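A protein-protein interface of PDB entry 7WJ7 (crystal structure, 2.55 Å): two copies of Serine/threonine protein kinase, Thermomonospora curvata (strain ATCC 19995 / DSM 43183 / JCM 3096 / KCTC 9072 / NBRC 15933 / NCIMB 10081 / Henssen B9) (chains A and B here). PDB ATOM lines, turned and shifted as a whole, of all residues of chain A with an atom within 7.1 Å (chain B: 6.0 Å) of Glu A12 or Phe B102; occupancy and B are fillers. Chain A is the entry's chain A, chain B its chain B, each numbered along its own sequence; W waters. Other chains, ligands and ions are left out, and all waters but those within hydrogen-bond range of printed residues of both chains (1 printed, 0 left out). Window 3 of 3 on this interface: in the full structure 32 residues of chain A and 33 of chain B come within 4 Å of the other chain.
Of the 10 printed residues of chain A, 5 touch a printed residue of chain B. Hydrophobic or aromatic side chains of chain A that line the printed part of chain B: Ile A11 and Ala A14. Of the 20 printed residues of chain B, 5 touch a printed residue of chain A.
No position is printed for both chains. Of the 9 pairs that touch across the chains among the printed residues, none has its exchanged pair printed and touching as well.
The backbone NH (N) of Glu A12 is in hydrogen-bond range of the backbone carbonyl oxygen (O) of Ala A25 (2.9 Å). The backbone NH of Arg A10 lies within hydrogen-bond range of the backbone carbonyl oxygen of Ile A27, at 3.2 Å. The backbone carbonyl oxygen (O) of Ala A13 lies within hydrogen-bond range of the backbone NH (N) of Ala A25. The backbone NH (N) of Asn B99 sits at hydrogen-bond distance from the backbone carbonyl oxygen (O) of Met B151 (3.3 Å).
Of the printed residues of chain A, Asn B99 touches Ala A14. Of chain A, only Glu A12 (3.8 Å) comes within 4 Å of Phe B102. Glu B104 touches none of the printed residues of chain A. Of the printed residues of chain A, Leu B213 touches Ile A11 (3.6 Å), Glu A12 (3.9 Å), Ala A13 (3.5 Å) and Ala A14 (3.7 Å). Of the printed residues of chain A, Thr B214 touches Arg A10 and Ile A11. The nearest residue of chain B that does not touch Glu A12 is Glu B104 (5.3 Å). The nearest printed residue of chain A that does not touch Phe B102 is Ala A13 (5.2 Å). The nearest printed residue of chain A that does not touch Asn B99 is Ala A13 (5.6 Å).
N of Ile A11 lies within hydrogen-bond range of OG1 of Thr B214. The backbone carbonyl oxygen of Ala A14 lies within hydrogen-bond range of the side-chain amide nitrogen of Asn B99, at 2.7 Å.
Among the printed residues, merely in contact across the chains: Glu A12 with Ala B103, Ala A13 with Leu B213, Ile A11 with Leu B213, Arg A10 with Thr B214, Ala A14 with Leu B213, Glu A12 with Phe B102 and Glu A12 with Leu B213.
Water W1 lies within hydrogen-bond range of O of Asn B99 (2.4 Å), N of Ala A14 (3.0 Å) and N of Ala B103 (3.4 Å).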
ATOM      1  N   ARG A  10      21.105 -16.142   3.252  1.00  0.00           N
ATOM      2  CA  ARG A  10      20.993 -17.402   3.978  1.00  0.00           C
ATOM      3  C   ARG A  10      19.670 -18.052   3.602  1.00  0.00           C
ATOM      4  O   ARG A  10      18.600 -17.567   3.985  1.00  0.00           O
ATOM      5  CB  ARG A  10      21.091 -17.190   5.486  1.00  0.00           C
ATOM      6  CG  ARG A  10      21.925 -18.254   6.180  1.00  0.00           C
ATOM      7  CD  ARG A  10      21.360 -18.623   7.544  1.00  0.00           C
ATOM      8  NE  ARG A  10      20.942 -17.451   8.304  1.00  0.00           N
ATOM      9  CZ  ARG A  10      21.769 -16.549   8.815  1.00  0.00           C
ATOM     10  NH1 ARG A  10      23.080 -16.648   8.668  1.00  0.00           N
ATOM     11  NH2 ARG A  10      21.267 -15.517   9.488  1.00  0.00           N
ATOM     12  N   ILE A  11      19.750 -19.146   2.846  1.00  0.00           N
ATOM     13  CA  ILE A  11      18.553 -19.861   2.425  1.00  0.00           C
ATOM     14  C   ILE A  11      17.952 -20.573   3.630  1.00  0.00           C
ATOM     15  O   ILE A  11      18.635 -21.335   4.326  1.00  0.00           O
ATOM     16  CB  ILE A  11      18.891 -20.847   1.296  1.00  0.00           C
ATOM     17  CG1 ILE A  11      19.825 -20.201   0.269  1.00  0.00           C
ATOM     18  CG2 ILE A  11      17.628 -21.288   0.589  1.00  0.00           C
ATOM     19  CD1 ILE A  11      19.294 -18.913  -0.331  1.00  0.00           C
ATOM     20  N   GLU A  12      16.671 -20.315   3.891  1.00  0.00           N
ATOM     21  CA  GLU A  12      15.979 -20.897   5.034  1.00  0.00           C
ATOM     22  C   GLU A  12      15.009 -22.009   4.670  1.00  0.00           C
ATOM     23  O   GLU A  12      14.773 -22.892   5.496  1.00  0.00           O
ATOM     24  CB  GLU A  12      15.214 -19.814   5.805  1.00  0.00           C
ATOM     25  CG  GLU A  12      16.081 -18.687   6.341  1.00  0.00           C
ATOM     26  CD  GLU A  12      15.479 -18.021   7.564  1.00  0.00           C
ATOM     27  OE1 GLU A  12      14.368 -17.459   7.453  1.00  0.00           O
ATOM     28  OE2 GLU A  12      16.116 -18.060   8.637  1.00  0.00           O
ATOM     29  N   ALA A  13      14.441 -21.992   3.467  1.00  0.00           N
ATOM     30  CA  ALA A  13      13.446 -22.983   3.089  1.00  0.00           C
ATOM     31  C   ALA A  13      13.496 -23.211   1.587  1.00  0.00           C
ATOM     32  O   ALA A  13      13.801 -22.300   0.813  1.00  0.00           O
ATOM     33  CB  ALA A  13      12.036 -22.552   3.511  1.00  0.00           C
ATOM     34  N   ALA A  14      13.198 -24.445   1.183  1.00  0.00           N
ATOM     35  CA  ALA A  14      13.096 -24.821  -0.223  1.00  0.00           C
ATOM     36  C   ALA A  14      11.618 -24.838  -0.593  1.00  0.00           C
ATOM     37  O   ALA A  14      10.863 -25.691  -0.114  1.00  0.00           O
ATOM     38  CB  ALA A  14      13.746 -26.180  -0.478  1.00  0.00           C
ATOM     39  N   TYR A  24      13.445 -20.442  -3.584  1.00  0.00           N
ATOM     40  CA  TYR A  24      13.825 -20.629  -2.194  1.00  0.00           C
ATOM     41  C   TYR A  24      13.557 -19.356  -1.408  1.00  0.00           C
ATOM     42  O   TYR A  24      13.651 -18.244  -1.937  1.00  0.00           O
ATOM     43  CB  TYR A  24      15.302 -21.019  -2.065  1.00  0.00           C
ATOM     44  CG  TYR A  24      15.666 -22.314  -2.759  1.00  0.00           C
ATOM     45  CD1 TYR A  24      15.890 -22.352  -4.128  1.00  0.00           C
ATOM     46  CD2 TYR A  24      15.785 -23.498  -2.042  1.00  0.00           C
ATOM     47  CE1 TYR A  24      16.221 -23.532  -4.768  1.00  0.00           C
ATOM     48  CE2 TYR A  24      16.116 -24.685  -2.673  1.00  0.00           C
ATOM     49  CZ  TYR A  24      16.333 -24.695  -4.036  1.00  0.00           C
ATOM     50  OH  TYR A  24      16.663 -25.871  -4.671  1.00  0.00           O
ATOM     51  N   ALA A  25      13.211 -19.535  -0.138  1.00  0.00           N
ATOM     52  CA  ALA A  25      13.014 -18.425   0.776  1.00  0.00           C
ATOM     53  C   ALA A  25      14.310 -18.152   1.522  1.00  0.00           C
ATOM     54  O   ALA A  25      15.037 -19.080   1.890  1.00  0.00           O
ATOM     55  CB  ALA A  25      11.882 -18.726   1.757  1.00  0.00           C
ATOM     56  N   GLY A  26      14.606 -16.873   1.729  1.00  0.00           N
ATOM     57  CA  GLY A  26      15.879 -16.496   2.298  1.00  0.00           C
ATOM     58  C   GLY A  26      15.778 -15.211   3.087  1.00  0.00           C
ATOM     59  O   GLY A  26      14.711 -14.607   3.207  1.00  0.00           O
ATOM     60  N   ILE A  27      16.920 -14.805   3.634  1.00  0.00           N
ATOM     61  CA  ILE A  27      17.049 -13.576   4.404  1.00  0.00           C
ATOM     62  C   ILE A  27      18.353 -12.906   3.994  1.00  0.00           C
ATOM     63  O   ILE A  27      19.407 -13.550   3.983  1.00  0.00           O
ATOM     64  CB  ILE A  27      17.034 -13.842   5.925  1.00  0.00           C
ATOM     65  CG1 ILE A  27      15.603 -13.844   6.470  1.00  0.00           C
ATOM     66  CG2 ILE A  27      17.881 -12.815   6.665  1.00  0.00           C
ATOM     67  CD1 ILE A  27      15.521 -14.180   7.949  1.00  0.00           C
ATOM     68  N   GLN A  34      13.550 -10.214   4.511  1.00  0.00           N
ATOM     69  CA  GLN A  34      13.067 -11.430   3.873  1.00  0.00           C
ATOM     70  C   GLN A  34      13.102 -11.279   2.357  1.00  0.00           C
ATOM     71  O   GLN A  34      12.642 -10.270   1.814  1.00  0.00           O
ATOM     72  CB  GLN A  34      11.647 -11.750   4.342  1.00  0.00           C
ATOM     73  CG  GLN A  34      11.536 -12.065   5.827  1.00  0.00           C
ATOM     74  CD  GLN A  34      11.629 -13.552   6.104  1.00  0.00           C
ATOM     75  OE1 GLN A  34      11.591 -14.368   5.181  1.00  0.00           O
ATOM     76  NE2 GLN A  34      11.751 -13.914   7.375  1.00  0.00           N
ATOM     77  N   LEU B  98      10.228 -34.112   1.227  1.00  0.00           N
ATOM     78  CA  LEU B  98      11.546 -34.065   1.853  1.00  0.00           C
ATOM     79  C   LEU B  98      12.090 -32.644   1.930  1.00  0.00           C
ATOM     80  O   LEU B  98      12.872 -32.329   2.834  1.00  0.00           O
ATOM     81  CB  LEU B  98      12.516 -34.967   1.088  1.00  0.00           C
ATOM     82  CG  LEU B  98      13.946 -35.092   1.614  1.00  0.00           C
ATOM     83  CD1 LEU B  98      13.944 -35.495   3.077  1.00  0.00           C
ATOM     84  CD2 LEU B  98      14.736 -36.087   0.781  1.00  0.00           C
ATOM     85  N   ASN B  99      11.686 -31.771   1.004  1.00  0.00           N
ATOM     86  CA  ASN B  99      12.239 -30.422   0.990  1.00  0.00           C
ATOM     87  C   ASN B  99      11.776 -29.604   2.186  1.00  0.00           C
ATOM     88  O   ASN B  99      12.457 -28.652   2.582  1.00  0.00           O
ATOM     89  CB  ASN B  99      11.882 -29.710  -0.316  1.00  0.00           C
ATOM     90  CG  ASN B  99      10.391 -29.476  -0.470  1.00  0.00           C
ATOM     91  OD1 ASN B  99       9.622 -30.416  -0.653  1.00  0.00           O
ATOM     92  ND2 ASN B  99       9.979 -28.215  -0.406  1.00  0.00           N
ATOM     93  N   THR B 100      10.634 -29.953   2.779  1.00  0.00           N
ATOM     94  CA  THR B 100      10.163 -29.234   3.954  1.00  0.00           C
ATOM     95  C   THR B 100      10.938 -29.593   5.214  1.00  0.00           C
ATOM     96  O   THR B 100      10.794 -28.897   6.224  1.00  0.00           O
ATOM     97  CB  THR B 100       8.673 -29.499   4.158  1.00  0.00           C
ATOM     98  OG1 THR B 100       8.490 -30.811   4.704  1.00  0.00           O
ATOM     99  CG2 THR B 100       7.940 -29.402   2.831  1.00  0.00           C
ATOM    100  N   PHE B 101      11.750 -30.651   5.183  1.00  0.00           N
ATOM    101  CA  PHE B 101      12.612 -30.966   6.315  1.00  0.00           C
ATOM    102  C   PHE B 101      13.843 -30.075   6.372  1.00  0.00           C
ATOM    103  O   PHE B 101      14.447 -29.938   7.440  1.00  0.00           O
ATOM    104  CB  PHE B 101      13.047 -32.433   6.266  1.00  0.00           C
ATOM    105  CG  PHE B 101      11.930 -33.408   6.506  1.00  0.00           C
ATOM    106  CD1 PHE B 101      11.099 -33.802   5.469  1.00  0.00           C
ATOM    107  CD2 PHE B 101      11.707 -33.925   7.770  1.00  0.00           C
ATOM    108  CE1 PHE B 101      10.069 -34.699   5.690  1.00  0.00           C
ATOM    109  CE2 PHE B 101      10.678 -34.821   7.998  1.00  0.00           C
ATOM    110  CZ  PHE B 101       9.859 -35.208   6.955  1.00  0.00           C
ATOM    111  N   PHE B 102      14.225 -29.466   5.254  1.00  0.00           N
ATOM    112  CA  PHE B 102      15.398 -28.603   5.224  1.00  0.00           C
ATOM    113  C   PHE B 102      15.137 -27.242   5.852  1.00  0.00           C
ATOM    114  O   PHE B 102      16.079 -26.459   6.011  1.00  0.00           O
ATOM    115  CB  PHE B 102      15.873 -28.436   3.778  1.00  0.00           C
ATOM    116  CG  PHE B 102      16.550 -29.660   3.218  1.00  0.00           C
ATOM    117  CD1 PHE B 102      15.874 -30.869   3.141  1.00  0.00           C
ATOM    118  CD2 PHE B 102      17.871 -29.610   2.805  1.00  0.00           C
ATOM    119  CE1 PHE B 102      16.492 -32.001   2.636  1.00  0.00           C
ATOM    120  CE2 PHE B 102      18.494 -30.737   2.289  1.00  0.00           C
ATOM    121  CZ  PHE B 102      17.803 -31.936   2.210  1.00  0.00           C
ATOM    122  N   ALA B 103      13.889 -26.944   6.214  1.00  0.00           N
ATOM    123  CA  ALA B 103      13.592 -25.685   6.883  1.00  0.00           C
ATOM    124  C   ALA B 103      14.109 -25.692   8.317  1.00  0.00           C
ATOM    125  O   ALA B 103      14.987 -24.899   8.677  1.00  0.00           O
ATOM    126  CB  ALA B 103      12.089 -25.415   6.851  1.00  0.00           C
ATOM    127  N   GLU B 104      13.598 -26.606   9.144  1.00  0.00           N
ATOM    128  CA  GLU B 104      13.925 -26.674  10.563  1.00  0.00           C
ATOM    129  C   GLU B 104      14.950 -27.755  10.886  1.00  0.00           C
ATOM    130  O   GLU B 104      15.909 -27.497  11.619  1.00  0.00           O
ATOM    131  CB  GLU B 104      12.647 -26.913  11.380  1.00  0.00           C
ATOM    132  N   ARG B 105      14.769 -28.963  10.349  1.00  0.00           N
ATOM    133  CA  ARG B 105      15.586 -30.114  10.725  1.00  0.00           C
ATOM    134  C   ARG B 105      17.043 -29.983  10.296  1.00  0.00           C
ATOM    135  O   ARG B 105      17.851 -30.874  10.576  1.00  0.00           O
ATOM    136  CB  ARG B 105      14.997 -31.395  10.126  1.00  0.00           C
ATOM    137  CG  ARG B 105      15.320 -32.675  10.886  1.00  0.00           C
ATOM    138  CD  ARG B 105      15.005 -33.887  10.019  1.00  0.00           C
ATOM    139  NE  ARG B 105      13.947 -34.724  10.567  1.00  0.00           N
ATOM    140  CZ  ARG B 105      14.126 -35.619  11.528  1.00  0.00           C
ATOM    141  NH1 ARG B 105      15.321 -35.837  12.053  1.00  0.00           N
ATOM    142  NH2 ARG B 105      13.084 -36.321  11.963  1.00  0.00           N
ATOM    143  N   HIS B 106      17.373 -28.879   9.617  1.00  0.00           N
ATOM    144  CA  HIS B 106      18.783 -28.658   9.193  1.00  0.00           C
ATOM    145  C   HIS B 106      19.533 -27.723  10.151  1.00  0.00           C
ATOM    146  O   HIS B 106      20.595 -28.142  10.622  1.00  0.00           O
ATOM    147  CB  HIS B 106      18.918 -28.393   7.686  1.00  0.00           C
ATOM    148  CG  HIS B 106      19.661 -29.481   6.990  1.00  0.00           C
ATOM    149  ND1 HIS B 106      19.168 -30.115   5.872  1.00  0.00           N
ATOM    150  CD2 HIS B 106      20.844 -30.069   7.269  1.00  0.00           C
ATOM    151  CE1 HIS B 106      20.025 -31.033   5.477  1.00  0.00           C
ATOM    152  NE2 HIS B 106      21.059 -31.028   6.319  1.00  0.00           N
ATOM    153  N   PRO B 107      19.104 -26.472  10.434  1.00  0.00           N
ATOM    154  CA  PRO B 107      19.789 -25.654  11.434  1.00  0.00           C
ATOM    155  C   PRO B 107      19.339 -26.060  12.844  1.00  0.00           C
ATOM    156  O   PRO B 107      20.175 -26.553  13.573  1.00  0.00           O
ATOM    157  CB  PRO B 107      19.341 -24.227  11.097  1.00  0.00           C
ATOM    158  CG  PRO B 107      17.958 -24.414  10.529  1.00  0.00           C
ATOM    159  CD  PRO B 107      18.039 -25.717   9.763  1.00  0.00           C
ATOM    160  N   TYR B 121      20.133 -38.033  13.424  1.00  0.00           N
ATOM    161  CA  TYR B 121      19.852 -37.506  12.093  1.00  0.00           C
ATOM    162  C   TYR B 121      20.555 -38.318  11.011  1.00  0.00           C
ATOM    163  O   TYR B 121      19.988 -38.547   9.936  1.00  0.00           O
ATOM    164  CB  TYR B 121      20.264 -36.038  11.998  1.00  0.00           C
ATOM    165  CG  TYR B 121      20.060 -35.476  10.612  1.00  0.00           C
ATOM    166  CD1 TYR B 121      18.799 -35.090  10.183  1.00  0.00           C
ATOM    167  CD2 TYR B 121      21.122 -35.357   9.724  1.00  0.00           C
ATOM    168  CE1 TYR B 121      18.599 -34.587   8.916  1.00  0.00           C
ATOM    169  CE2 TYR B 121      20.930 -34.855   8.449  1.00  0.00           C
ATOM    170  CZ  TYR B 121      19.667 -34.472   8.053  1.00  0.00           C
ATOM    171  OH  TYR B 121      19.465 -33.969   6.789  1.00  0.00           O
ATOM    172  N   MET B 151      14.536 -33.695  -3.825  1.00  0.00           N
ATOM    173  CA  MET B 151      13.884 -33.503  -2.533  1.00  0.00           C
ATOM    174  C   MET B 151      12.411 -33.133  -2.671  1.00  0.00           C
ATOM    175  O   MET B 151      11.608 -33.452  -1.788  1.00  0.00           O
ATOM    176  CB  MET B 151      14.635 -32.424  -1.751  1.00  0.00           C
ATOM    177  CG  MET B 151      15.049 -31.253  -2.633  1.00  0.00           C
ATOM    178  SD  MET B 151      16.091 -29.993  -1.873  1.00  0.00           S
ATOM    179  CE  MET B 151      15.569 -30.058  -0.176  1.00  0.00           C
ATOM    180  N   ALA B 208      23.142 -34.148  -0.478  1.00  0.00           N
ATOM    181  CA  ALA B 208      22.169 -33.105  -0.165  1.00  0.00           C
ATOM    182  C   ALA B 208      21.532 -33.324   1.202  1.00  0.00           C
ATOM    183  O   ALA B 208      21.227 -32.358   1.911  1.00  0.00           O
ATOM    184  CB  ALA B 208      21.097 -33.047  -1.253  1.00  0.00           C
ATOM    185  N   LEU B 209      21.332 -34.586   1.592  1.00  0.00           N
ATOM    186  CA  LEU B 209      20.724 -34.892   2.883  1.00  0.00           C
ATOM    187  C   LEU B 209      21.533 -34.343   4.050  1.00  0.00           C
ATOM    188  O   LEU B 209      20.985 -34.168   5.143  1.00  0.00           O
ATOM    189  CB  LEU B 209      20.557 -36.404   3.032  1.00  0.00           C
ATOM    190  CG  LEU B 209      19.287 -37.009   2.435  1.00  0.00           C
ATOM    191  CD1 LEU B 209      19.462 -38.500   2.201  1.00  0.00           C
ATOM    192  CD2 LEU B 209      18.100 -36.748   3.350  1.00  0.00           C
ATOM    193  N   PHE B 210      22.817 -34.060   3.842  1.00  0.00           N
ATOM    194  CA  PHE B 210      23.688 -33.586   4.904  1.00  0.00           C
ATOM    195  C   PHE B 210      24.145 -32.147   4.720  1.00  0.00           C
ATOM    196  O   PHE B 210      24.689 -31.563   5.664  1.00  0.00           O
ATOM    197  CB  PHE B 210      24.920 -34.494   5.010  1.00  0.00           C
ATOM    198  CG  PHE B 210      24.596 -35.908   5.390  1.00  0.00           C
ATOM    199  CD1 PHE B 210      24.162 -36.214   6.670  1.00  0.00           C
ATOM    200  CD2 PHE B 210      24.711 -36.932   4.463  1.00  0.00           C
ATOM    201  CE1 PHE B 210      23.860 -37.516   7.023  1.00  0.00           C
ATOM    202  CE2 PHE B 210      24.408 -38.237   4.809  1.00  0.00           C
ATOM    203  CZ  PHE B 210      23.982 -38.528   6.091  1.00  0.00           C
ATOM    204  N   LEU B 211      23.947 -31.567   3.552  1.00  0.00           N
ATOM    205  CA  LEU B 211      24.473 -30.219   3.406  1.00  0.00           C
ATOM    206  C   LEU B 211      23.413 -29.180   3.751  1.00  0.00           C
ATOM    207  O   LEU B 211      22.222 -29.388   3.496  1.00  0.00           O
ATOM    208  CB  LEU B 211      24.965 -29.989   1.981  1.00  0.00           C
ATOM    209  CG  LEU B 211      26.201 -30.804   1.607  1.00  0.00           C
ATOM    210  CD1 LEU B 211      26.428 -30.790   0.105  1.00  0.00           C
ATOM    211  CD2 LEU B 211      27.410 -30.272   2.355  1.00  0.00           C
ATOM    212  N   PRO B 212      23.825 -28.061   4.342  1.00  0.00           N
ATOM    213  CA  PRO B 212      22.874 -26.969   4.582  1.00  0.00           C
ATOM    214  C   PRO B 212      22.443 -26.322   3.274  1.00  0.00           C
ATOM    215  O   PRO B 212      23.161 -26.352   2.270  1.00  0.00           O
ATOM    216  CB  PRO B 212      23.658 -25.988   5.465  1.00  0.00           C
ATOM    217  CG  PRO B 212      25.093 -26.345   5.294  1.00  0.00           C
ATOM    218  CD  PRO B 212      25.171 -27.778   4.870  1.00  0.00           C
ATOM    219  N   LEU B 213      21.249 -25.724   3.308  1.00  0.00           N
ATOM    220  CA  LEU B 213      20.584 -25.263   2.091  1.00  0.00           C
ATOM    221  C   LEU B 213      21.454 -24.290   1.302  1.00  0.00           C
ATOM    222  O   LEU B 213      21.587 -24.411   0.078  1.00  0.00           O
ATOM    223  CB  LEU B 213      19.247 -24.616   2.459  1.00  0.00           C
ATOM    224  CG  LEU B 213      17.973 -25.366   2.064  1.00  0.00           C
ATOM    225  CD1 LEU B 213      16.766 -24.446   2.122  1.00  0.00           C
ATOM    226  CD2 LEU B 213      18.112 -25.970   0.674  1.00  0.00           C
ATOM    227  N   THR B 214      22.059 -23.320   1.991  1.00  0.00           N
ATOM    228  CA  THR B 214      22.852 -22.301   1.307  1.00  0.00           C
ATOM    229  C   THR B 214      24.037 -22.921   0.577  1.00  0.00           C
ATOM    230  O   THR B 214      24.275 -22.632  -0.601  1.00  0.00           O
ATOM    231  CB  THR B 214      23.325 -21.248   2.309  1.00  0.00           C
ATOM    232  OG1 THR B 214      22.189 -20.658   2.954  1.00  0.00           O
ATOM    233  CG2 THR B 214      24.121 -20.159   1.602  1.00  0.00           C
ATOM    234  N   LEU B 216      24.238 -25.928  -0.361  1.00  0.00           N
ATOM    235  CA  LEU B 216      23.703 -26.809  -1.393  1.00  0.00           C
ATOM    236  C   LEU B 216      23.628 -26.090  -2.734  1.00  0.00           C
ATOM    237  O   LEU B 216      24.126 -26.588  -3.751  1.00  0.00           O
ATOM    238  CB  LEU B 216      22.321 -27.317  -0.980  1.00  0.00           C
ATOM    239  CG  LEU B 216      22.186 -28.790  -0.597  1.00  0.00           C
ATOM    240  CD1 LEU B 216      20.809 -29.067  -0.008  1.00  0.00           C
ATOM    241  CD2 LEU B 216      22.455 -29.678  -1.790  1.00  0.00           C
HETATM  242  O   HOH W   1      12.205 -26.367   3.306  1.00  0.00           O
